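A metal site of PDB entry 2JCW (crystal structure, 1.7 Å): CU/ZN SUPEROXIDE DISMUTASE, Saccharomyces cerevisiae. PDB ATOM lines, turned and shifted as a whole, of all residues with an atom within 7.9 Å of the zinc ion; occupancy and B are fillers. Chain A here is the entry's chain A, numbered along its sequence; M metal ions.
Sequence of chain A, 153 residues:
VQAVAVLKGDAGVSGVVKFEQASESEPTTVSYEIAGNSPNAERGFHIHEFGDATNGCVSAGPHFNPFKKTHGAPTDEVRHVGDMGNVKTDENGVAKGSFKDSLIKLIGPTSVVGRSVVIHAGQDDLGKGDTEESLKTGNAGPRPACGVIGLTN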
ATOM      1  N   PHE A  45       0.402  36.295 -10.174  1.00  0.00           N
ATOM      2  CA  PHE A  45      -1.056  36.431 -10.336  1.00  0.00           C
ATOM      3  C   PHE A  45      -1.692  35.063 -10.030  1.00  0.00           C
ATOM      4  O   PHE A  45      -1.452  34.093 -10.763  1.00  0.00           O
ATOM      5  CB  PHE A  45      -1.271  36.836 -11.809  1.00  0.00           C
ATOM      6  CG  PHE A  45      -2.671  37.218 -12.176  1.00  0.00           C
ATOM      7  CD1 PHE A  45      -3.422  38.087 -11.374  1.00  0.00           C
ATOM      8  CD2 PHE A  45      -3.223  36.789 -13.370  1.00  0.00           C
ATOM      9  CE1 PHE A  45      -4.697  38.510 -11.763  1.00  0.00           C
ATOM     10  CE2 PHE A  45      -4.492  37.207 -13.771  1.00  0.00           C
ATOM     11  CZ  PHE A  45      -5.230  38.075 -12.963  1.00  0.00           C
ATOM     12  N   HIS A  46      -2.477  34.954  -8.956  1.00  0.00           N
ATOM     13  CA  HIS A  46      -3.065  33.646  -8.626  1.00  0.00           C
ATOM     14  C   HIS A  46      -4.445  33.725  -8.012  1.00  0.00           C
ATOM     15  O   HIS A  46      -4.861  34.765  -7.501  1.00  0.00           O
ATOM     16  CB  HIS A  46      -2.215  32.876  -7.594  1.00  0.00           C
ATOM     17  CG  HIS A  46      -0.742  33.127  -7.703  1.00  0.00           C
ATOM     18  ND1 HIS A  46      -0.054  33.873  -6.778  1.00  0.00           N
ATOM     19  CD2 HIS A  46       0.160  32.722  -8.626  1.00  0.00           C
ATOM     20  CE1 HIS A  46       1.227  33.924  -7.133  1.00  0.00           C
ATOM     21  NE2 HIS A  46       1.372  33.236  -8.248  1.00  0.00           N
ATOM     22  N   ILE A  47      -5.092  32.573  -7.997  1.00  0.00           N
ATOM     23  CA  ILE A  47      -6.378  32.429  -7.349  1.00  0.00           C
ATOM     24  C   ILE A  47      -6.058  31.758  -6.012  1.00  0.00           C
ATOM     25  O   ILE A  47      -5.333  30.764  -5.951  1.00  0.00           O
ATOM     26  CB  ILE A  47      -7.367  31.588  -8.165  1.00  0.00           C
ATOM     27  CG1 ILE A  47      -7.702  32.364  -9.443  1.00  0.00           C
ATOM     28  CG2 ILE A  47      -8.646  31.333  -7.344  1.00  0.00           C
ATOM     29  CD1 ILE A  47      -8.500  31.579 -10.439  1.00  0.00           C
ATOM     30  N   HIS A  48      -6.423  32.441  -4.933  1.00  0.00           N
ATOM     31  CA  HIS A  48      -6.203  31.966  -3.589  1.00  0.00           C
ATOM     32  C   HIS A  48      -7.479  31.305  -3.097  1.00  0.00           C
ATOM     33  O   HIS A  48      -8.586  31.621  -3.579  1.00  0.00           O
ATOM     34  CB  HIS A  48      -5.757  33.120  -2.692  1.00  0.00           C
ATOM     35  CG  HIS A  48      -4.346  33.540  -2.923  1.00  0.00           C
ATOM     36  ND1 HIS A  48      -3.405  33.582  -1.921  1.00  0.00           N
ATOM     37  CD2 HIS A  48      -3.709  33.898  -4.060  1.00  0.00           C
ATOM     38  CE1 HIS A  48      -2.238  33.943  -2.430  1.00  0.00           C
ATOM     39  NE2 HIS A  48      -2.395  34.144  -3.718  1.00  0.00           N
ATOM     40  N   PRO A  62      -3.893  30.604   1.147  1.00  0.00           N
ATOM     41  CA  PRO A  62      -2.909  30.067   0.200  1.00  0.00           C
ATOM     42  C   PRO A  62      -3.473  29.918  -1.212  1.00  0.00           C
ATOM     43  O   PRO A  62      -4.654  30.206  -1.444  1.00  0.00           O
ATOM     44  CB  PRO A  62      -2.594  28.702   0.795  1.00  0.00           C
ATOM     45  CG  PRO A  62      -3.957  28.268   1.271  1.00  0.00           C
ATOM     46  CD  PRO A  62      -4.486  29.512   1.955  1.00  0.00           C
ATOM     47  N   HIS A  63      -2.633  29.510  -2.155  1.00  0.00           N
ATOM     48  CA  HIS A  63      -3.105  29.300  -3.523  1.00  0.00           C
ATOM     49  C   HIS A  63      -4.137  28.178  -3.513  1.00  0.00           C
ATOM     50  O   HIS A  63      -3.989  27.197  -2.785  1.00  0.00           O
ATOM     51  CB  HIS A  63      -1.960  28.897  -4.438  1.00  0.00           C
ATOM     52  CG  HIS A  63      -0.903  29.945  -4.572  1.00  0.00           C
ATOM     53  ND1 HIS A  63       0.213  29.787  -5.365  1.00  0.00           N
ATOM     54  CD2 HIS A  63      -0.784  31.164  -3.992  1.00  0.00           C
ATOM     55  CE1 HIS A  63       0.970  30.863  -5.263  1.00  0.00           C
ATOM     56  NE2 HIS A  63       0.382  31.712  -4.441  1.00  0.00           N
ATOM     57  N   PHE A  64      -5.174  28.339  -4.326  1.00  0.00           N
ATOM     58  CA  PHE A  64      -6.227  27.344  -4.444  1.00  0.00           C
ATOM     59  C   PHE A  64      -5.550  26.072  -4.971  1.00  0.00           C
ATOM     60  O   PHE A  64      -5.011  26.062  -6.092  1.00  0.00           O
ATOM     61  CB  PHE A  64      -7.321  27.834  -5.381  1.00  0.00           C
ATOM     62  CG  PHE A  64      -8.492  26.893  -5.477  1.00  0.00           C
ATOM     63  CD1 PHE A  64      -9.023  26.301  -4.330  1.00  0.00           C
ATOM     64  CD2 PHE A  64      -9.057  26.595  -6.705  1.00  0.00           C
ATOM     65  CE1 PHE A  64     -10.105  25.420  -4.407  1.00  0.00           C
ATOM     66  CE2 PHE A  64     -10.146  25.710  -6.801  1.00  0.00           C
ATOM     67  CZ  PHE A  64     -10.662  25.127  -5.650  1.00  0.00           C
ATOM     68  N   ASN A  65      -5.610  25.003  -4.191  1.00  0.00           N
ATOM     69  CA  ASN A  65      -4.905  23.762  -4.517  1.00  0.00           C
ATOM     70  C   ASN A  65      -5.697  22.548  -4.022  1.00  0.00           C
ATOM     71  O   ASN A  65      -5.238  21.805  -3.155  1.00  0.00           O
ATOM     72  CB  ASN A  65      -3.553  23.865  -3.800  1.00  0.00           C
ATOM     73  CG  ASN A  65      -2.610  22.730  -4.095  1.00  0.00           C
ATOM     74  OD1 ASN A  65      -2.634  22.124  -5.165  1.00  0.00           O
ATOM     75  ND2 ASN A  65      -1.695  22.521  -3.172  1.00  0.00           N
ATOM     76  N   LYS A  69      -1.015  19.694  -5.079  1.00  0.00           N
ATOM     77  CA  LYS A  69       0.183  19.633  -5.879  1.00  0.00           C
ATOM     78  C   LYS A  69       1.094  20.790  -5.460  1.00  0.00           C
ATOM     79  O   LYS A  69       0.735  21.567  -4.567  1.00  0.00           O
ATOM     80  CB  LYS A  69      -0.180  19.707  -7.358  1.00  0.00           C
ATOM     81  CG  LYS A  69      -1.015  18.513  -7.809  1.00  0.00           C
ATOM     82  CD  LYS A  69      -0.747  18.152  -9.245  1.00  0.00           C
ATOM     83  CE  LYS A  69      -1.487  16.874  -9.659  1.00  0.00           C
ATOM     84  NZ  LYS A  69      -1.184  15.721  -8.746  1.00  0.00           N
ATOM     85  N   THR A  70       2.289  20.848  -6.035  1.00  0.00           N
ATOM     86  CA  THR A  70       3.200  21.932  -5.720  1.00  0.00           C
ATOM     87  C   THR A  70       2.957  23.087  -6.688  1.00  0.00           C
ATOM     88  O   THR A  70       2.273  22.940  -7.708  1.00  0.00           O
ATOM     89  CB  THR A  70       4.691  21.498  -5.789  1.00  0.00           C
ATOM     90  OG1 THR A  70       4.957  20.832  -7.030  1.00  0.00           O
ATOM     91  CG2 THR A  70       5.029  20.585  -4.614  1.00  0.00           C
ATOM     92  N   HIS A  71       3.498  24.241  -6.338  1.00  0.00           N
ATOM     93  CA  HIS A  71       3.373  25.456  -7.123  1.00  0.00           C
ATOM     94  C   HIS A  71       4.133  25.339  -8.445  1.00  0.00           C
ATOM     95  O   HIS A  71       5.240  24.813  -8.462  1.00  0.00           O
ATOM     96  CB  HIS A  71       3.931  26.626  -6.304  1.00  0.00           C
ATOM     97  CG  HIS A  71       3.908  27.932  -7.027  1.00  0.00           C
ATOM     98  ND1 HIS A  71       2.760  28.698  -7.133  1.00  0.00           N
ATOM     99  CD2 HIS A  71       4.861  28.571  -7.732  1.00  0.00           C
ATOM    100  CE1 HIS A  71       3.024  29.753  -7.877  1.00  0.00           C
ATOM    101  NE2 HIS A  71       4.289  29.696  -8.246  1.00  0.00           N
ATOM    102  N   GLY A  72       3.537  25.823  -9.533  1.00  0.00           N
ATOM    103  CA  GLY A  72       4.195  25.778 -10.832  1.00  0.00           C
ATOM    104  C   GLY A  72       3.686  26.861 -11.774  1.00  0.00           C
ATOM    105  O   GLY A  72       3.016  27.802 -11.354  1.00  0.00           O
ATOM    106  N   ALA A  73       4.097  26.753 -13.034  1.00  0.00           N
ATOM    107  CA  ALA A  73       3.676  27.682 -14.073  1.00  0.00           C
ATOM    108  C   ALA A  73       2.333  27.175 -14.600  1.00  0.00           C
ATOM    109  O   ALA A  73       2.031  26.002 -14.469  1.00  0.00           O
ATOM    110  CB  ALA A  73       4.704  27.712 -15.200  1.00  0.00           C
ATOM    111  N   ARG A  79       1.002  21.840 -10.973  1.00  0.00           N
ATOM    112  CA  ARG A  79       0.765  23.222 -10.579  1.00  0.00           C
ATOM    113  C   ARG A  79      -0.455  23.221  -9.681  1.00  0.00           C
ATOM    114  O   ARG A  79      -1.170  22.217  -9.575  1.00  0.00           O
ATOM    115  CB  ARG A  79       0.468  24.077 -11.812  1.00  0.00           C
ATOM    116  CG  ARG A  79      -0.686  23.550 -12.665  1.00  0.00           C
ATOM    117  CD  ARG A  79      -1.122  24.528 -13.731  1.00  0.00           C
ATOM    118  NE  ARG A  79      -2.208  25.367 -13.244  1.00  0.00           N
ATOM    119  CZ  ARG A  79      -3.113  25.957 -14.022  1.00  0.00           C
ATOM    120  NH1 ARG A  79      -3.035  25.812 -15.336  1.00  0.00           N
ATOM    121  NH2 ARG A  79      -4.133  26.622 -13.502  1.00  0.00           N
ATOM    122  N   HIS A  80      -0.676  24.332  -8.996  1.00  0.00           N
ATOM    123  CA  HIS A  80      -1.859  24.484  -8.166  1.00  0.00           C
ATOM    124  C   HIS A  80      -2.944  24.897  -9.177  1.00  0.00           C
ATOM    125  O   HIS A  80      -2.614  25.518 -10.191  1.00  0.00           O
ATOM    126  CB  HIS A  80      -1.676  25.632  -7.160  1.00  0.00           C
ATOM    127  CG  HIS A  80      -0.623  25.372  -6.126  1.00  0.00           C
ATOM    128  ND1 HIS A  80       0.150  26.383  -5.582  1.00  0.00           N
ATOM    129  CD2 HIS A  80      -0.288  24.247  -5.459  1.00  0.00           C
ATOM    130  CE1 HIS A  80       0.902  25.882  -4.613  1.00  0.00           C
ATOM    131  NE2 HIS A  80       0.650  24.591  -4.520  1.00  0.00           N
ATOM    132  N   VAL A  81      -4.205  24.614  -8.911  1.00  0.00           N
ATOM    133  CA  VAL A  81      -5.275  25.051  -9.825  1.00  0.00           C
ATOM    134  C   VAL A  81      -5.239  26.586  -9.976  1.00  0.00           C
ATOM    135  O   VAL A  81      -5.426  27.103 -11.081  1.00  0.00           O
ATOM    136  CB  VAL A  81      -6.681  24.633  -9.292  1.00  0.00           C
ATOM    137  CG1 VAL A  81      -7.795  25.388 -10.028  1.00  0.00           C
ATOM    138  CG2 VAL A  81      -6.865  23.129  -9.440  1.00  0.00           C
ATOM    139  N   GLY A  82      -4.961  27.282  -8.878  1.00  0.00           N
ATOM    140  CA  GLY A  82      -4.931  28.738  -8.902  1.00  0.00           C
ATOM    141  C   GLY A  82      -3.720  29.443  -9.510  1.00  0.00           C
ATOM    142  O   GLY A  82      -3.690  30.672  -9.584  1.00  0.00           O
ATOM    143  N   ASP A  83      -2.742  28.680  -9.961  1.00  0.00           N
ATOM    144  CA  ASP A  83      -1.531  29.255 -10.542  1.00  0.00           C
ATOM    145  C   ASP A  83      -1.740  29.852 -11.938  1.00  0.00           C
ATOM    146  O   ASP A  83      -1.939  29.127 -12.929  1.00  0.00           O
ATOM    147  CB  ASP A  83      -0.402  28.218 -10.578  1.00  0.00           C
ATOM    148  CG  ASP A  83       0.114  27.866  -9.206  1.00  0.00           C
ATOM    149  OD1 ASP A  83      -0.130  28.586  -8.202  1.00  0.00           O
ATOM    150  OD2 ASP A  83       0.794  26.838  -9.079  1.00  0.00           O
ATOM    151  N   MET A  84      -1.672  31.175 -12.024  1.00  0.00           N
ATOM    152  CA  MET A  84      -1.832  31.881 -13.298  1.00  0.00           C
ATOM    153  C   MET A  84      -0.529  32.533 -13.766  1.00  0.00           C
ATOM    154  O   MET A  84      -0.525  33.284 -14.729  1.00  0.00           O
ATOM    155  CB  MET A  84      -2.984  32.905 -13.217  1.00  0.00           C
ATOM    156  CG  MET A  84      -4.314  32.254 -12.914  1.00  0.00           C
ATOM    157  SD  MET A  84      -5.682  33.406 -12.954  1.00  0.00           S
ATOM    158  CE  MET A  84      -5.403  34.338 -11.449  1.00  0.00           C
ATOM    159  N   GLY A  85       0.578  32.192 -13.114  1.00  0.00           N
ATOM    160  CA  GLY A  85       1.877  32.719 -13.500  1.00  0.00           C
ATOM    161  C   GLY A  85       2.114  34.195 -13.225  1.00  0.00           C
ATOM    162  O   GLY A  85       1.684  34.718 -12.197  1.00  0.00           O
ATOM    163  N   ASP A 124       6.774  35.839  -9.731  1.00  0.00           N
ATOM    164  CA  ASP A 124       6.559  34.445  -9.380  1.00  0.00           C
ATOM    165  C   ASP A 124       7.718  33.657 -10.035  1.00  0.00           C
ATOM    166  O   ASP A 124       7.943  33.777 -11.241  1.00  0.00           O
ATOM    167  CB  ASP A 124       5.205  34.029  -9.965  1.00  0.00           C
ATOM    168  CG  ASP A 124       4.763  32.642  -9.542  1.00  0.00           C
ATOM    169  OD1 ASP A 124       5.601  31.795  -9.185  1.00  0.00           O
ATOM    170  OD2 ASP A 124       3.549  32.388  -9.615  1.00  0.00           O
ATOM    171  N   GLY A 127       7.921  28.073  -9.239  1.00  0.00           N
ATOM    172  CA  GLY A 127       8.310  26.816  -8.618  1.00  0.00           C
ATOM    173  C   GLY A 127       9.678  26.320  -9.064  1.00  0.00           C
ATOM    174  O   GLY A 127      10.053  25.171  -8.776  1.00  0.00           O
ATOM    175  N   SER A 134       9.524  28.255  -2.958  1.00  0.00           N
ATOM    176  CA  SER A 134       9.266  28.300  -4.383  1.00  0.00           C
ATOM    177  C   SER A 134       8.140  27.329  -4.729  1.00  0.00           C
ATOM    178  O   SER A 134       7.296  27.620  -5.575  1.00  0.00           O
ATOM    179  CB  SER A 134      10.534  27.919  -5.131  1.00  0.00           C
ATOM    180  OG  SER A 134      10.305  27.874  -6.515  1.00  0.00           O
ATOM    181  N   LEU A 135       8.119  26.186  -4.067  1.00  0.00           N
ATOM    182  CA  LEU A 135       7.115  25.163  -4.317  1.00  0.00           C
ATOM    183  C   LEU A 135       5.773  25.427  -3.659  1.00  0.00           C
ATOM    184  O   LEU A 135       4.820  24.662  -3.862  1.00  0.00           O
ATOM    185  CB  LEU A 135       7.628  23.798  -3.861  1.00  0.00           C
ATOM    186  CG  LEU A 135       8.852  23.261  -4.593  1.00  0.00           C
ATOM    187  CD1 LEU A 135       9.265  21.937  -3.967  1.00  0.00           C
ATOM    188  CD2 LEU A 135       8.529  23.113  -6.072  1.00  0.00           C
ATOM    189  N   LYS A 136       5.694  26.490  -2.853  1.00  0.00           N
ATOM    190  CA  LYS A 136       4.457  26.823  -2.171  1.00  0.00           C
ATOM    191  C   LYS A 136       3.838  28.101  -2.711  1.00  0.00           C
ATOM    192  O   LYS A 136       2.662  28.124  -3.085  1.00  0.00           O
ATOM    193  CB  LYS A 136       4.677  26.993  -0.658  1.00  0.00           C
ATOM    194  CG  LYS A 136       5.567  25.954  -0.008  1.00  0.00           C
ATOM    195  CD  LYS A 136       4.964  24.557  -0.067  1.00  0.00           C
ATOM    196  CE  LYS A 136       5.925  23.485   0.488  1.00  0.00           C
ATOM    197  NZ  LYS A 136       7.140  23.254  -0.370  1.00  0.00           N
ATOM    198  N   THR A 137       4.640  29.156  -2.795  1.00  0.00           N
ATOM    199  CA  THR A 137       4.139  30.454  -3.253  1.00  0.00           C
ATOM    200  C   THR A 137       4.815  31.015  -4.501  1.00  0.00           C
ATOM    201  O   THR A 137       4.331  31.996  -5.083  1.00  0.00           O
ATOM    202  CB  THR A 137       4.290  31.509  -2.150  1.00  0.00           C
ATOM    203  OG1 THR A 137       5.684  31.761  -1.948  1.00  0.00           O
ATOM    204  CG2 THR A 137       3.703  31.023  -0.830  1.00  0.00           C
ATOM    205  N   GLY A 138       5.919  30.407  -4.913  1.00  0.00           N
ATOM    206  CA  GLY A 138       6.644  30.923  -6.061  1.00  0.00           C
ATOM    207  C   GLY A 138       7.441  32.160  -5.671  1.00  0.00           C
ATOM    208  O   GLY A 138       7.938  32.870  -6.548  1.00  0.00           O
HETATM  209 ZN    ZN M   1       0.679  28.255  -6.573  1.00  0.00          ZN
HETATM  210 CU    CU M   2      -0.830  34.576  -4.997  1.00  0.00          CU
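The backbone NH of Gly 72 lies within hydrogen-bond range of the side-chain carboxylate of Asp 83 (3.0 Å).
NH2 of Arg 79 is in hydrogen-bond range of O of Asp 83, 3.4 Å away.
A ring nitrogen (NE2) of His 63 sits close to a ring nitrogen (ND1) of His 46, 3.2 Å away.
NE2 of His 80 sits close to ND2 of Asn 65 (3.4 Å).
The backbone carbonyl oxygen of Lys 69 lies close to a ring nitrogen (NE2) of His 80, 3.0 Å away.
NE2 of His 71 is in hydrogen-bond range of OD1 of Asp 124 (2.6 Å).
N of His 71 sits at hydrogen-bond distance from O of Leu 135, at 2.8 Å.
The nearest printed residue that does not touch the zinc ion is Lys 136 (4.01 Å).
The zinc ion is bound by the side-chain carboxylate of Asp 83 (1.8 Å), a ring nitrogen (ND1) of His 63 (2.0 Å), a ring nitrogen (ND1) of His 80 (2.2 Å) and a ring nitrogen (ND1) of His 71 (2.2 Å).
The zinc ion has four donor atoms within binding distance.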
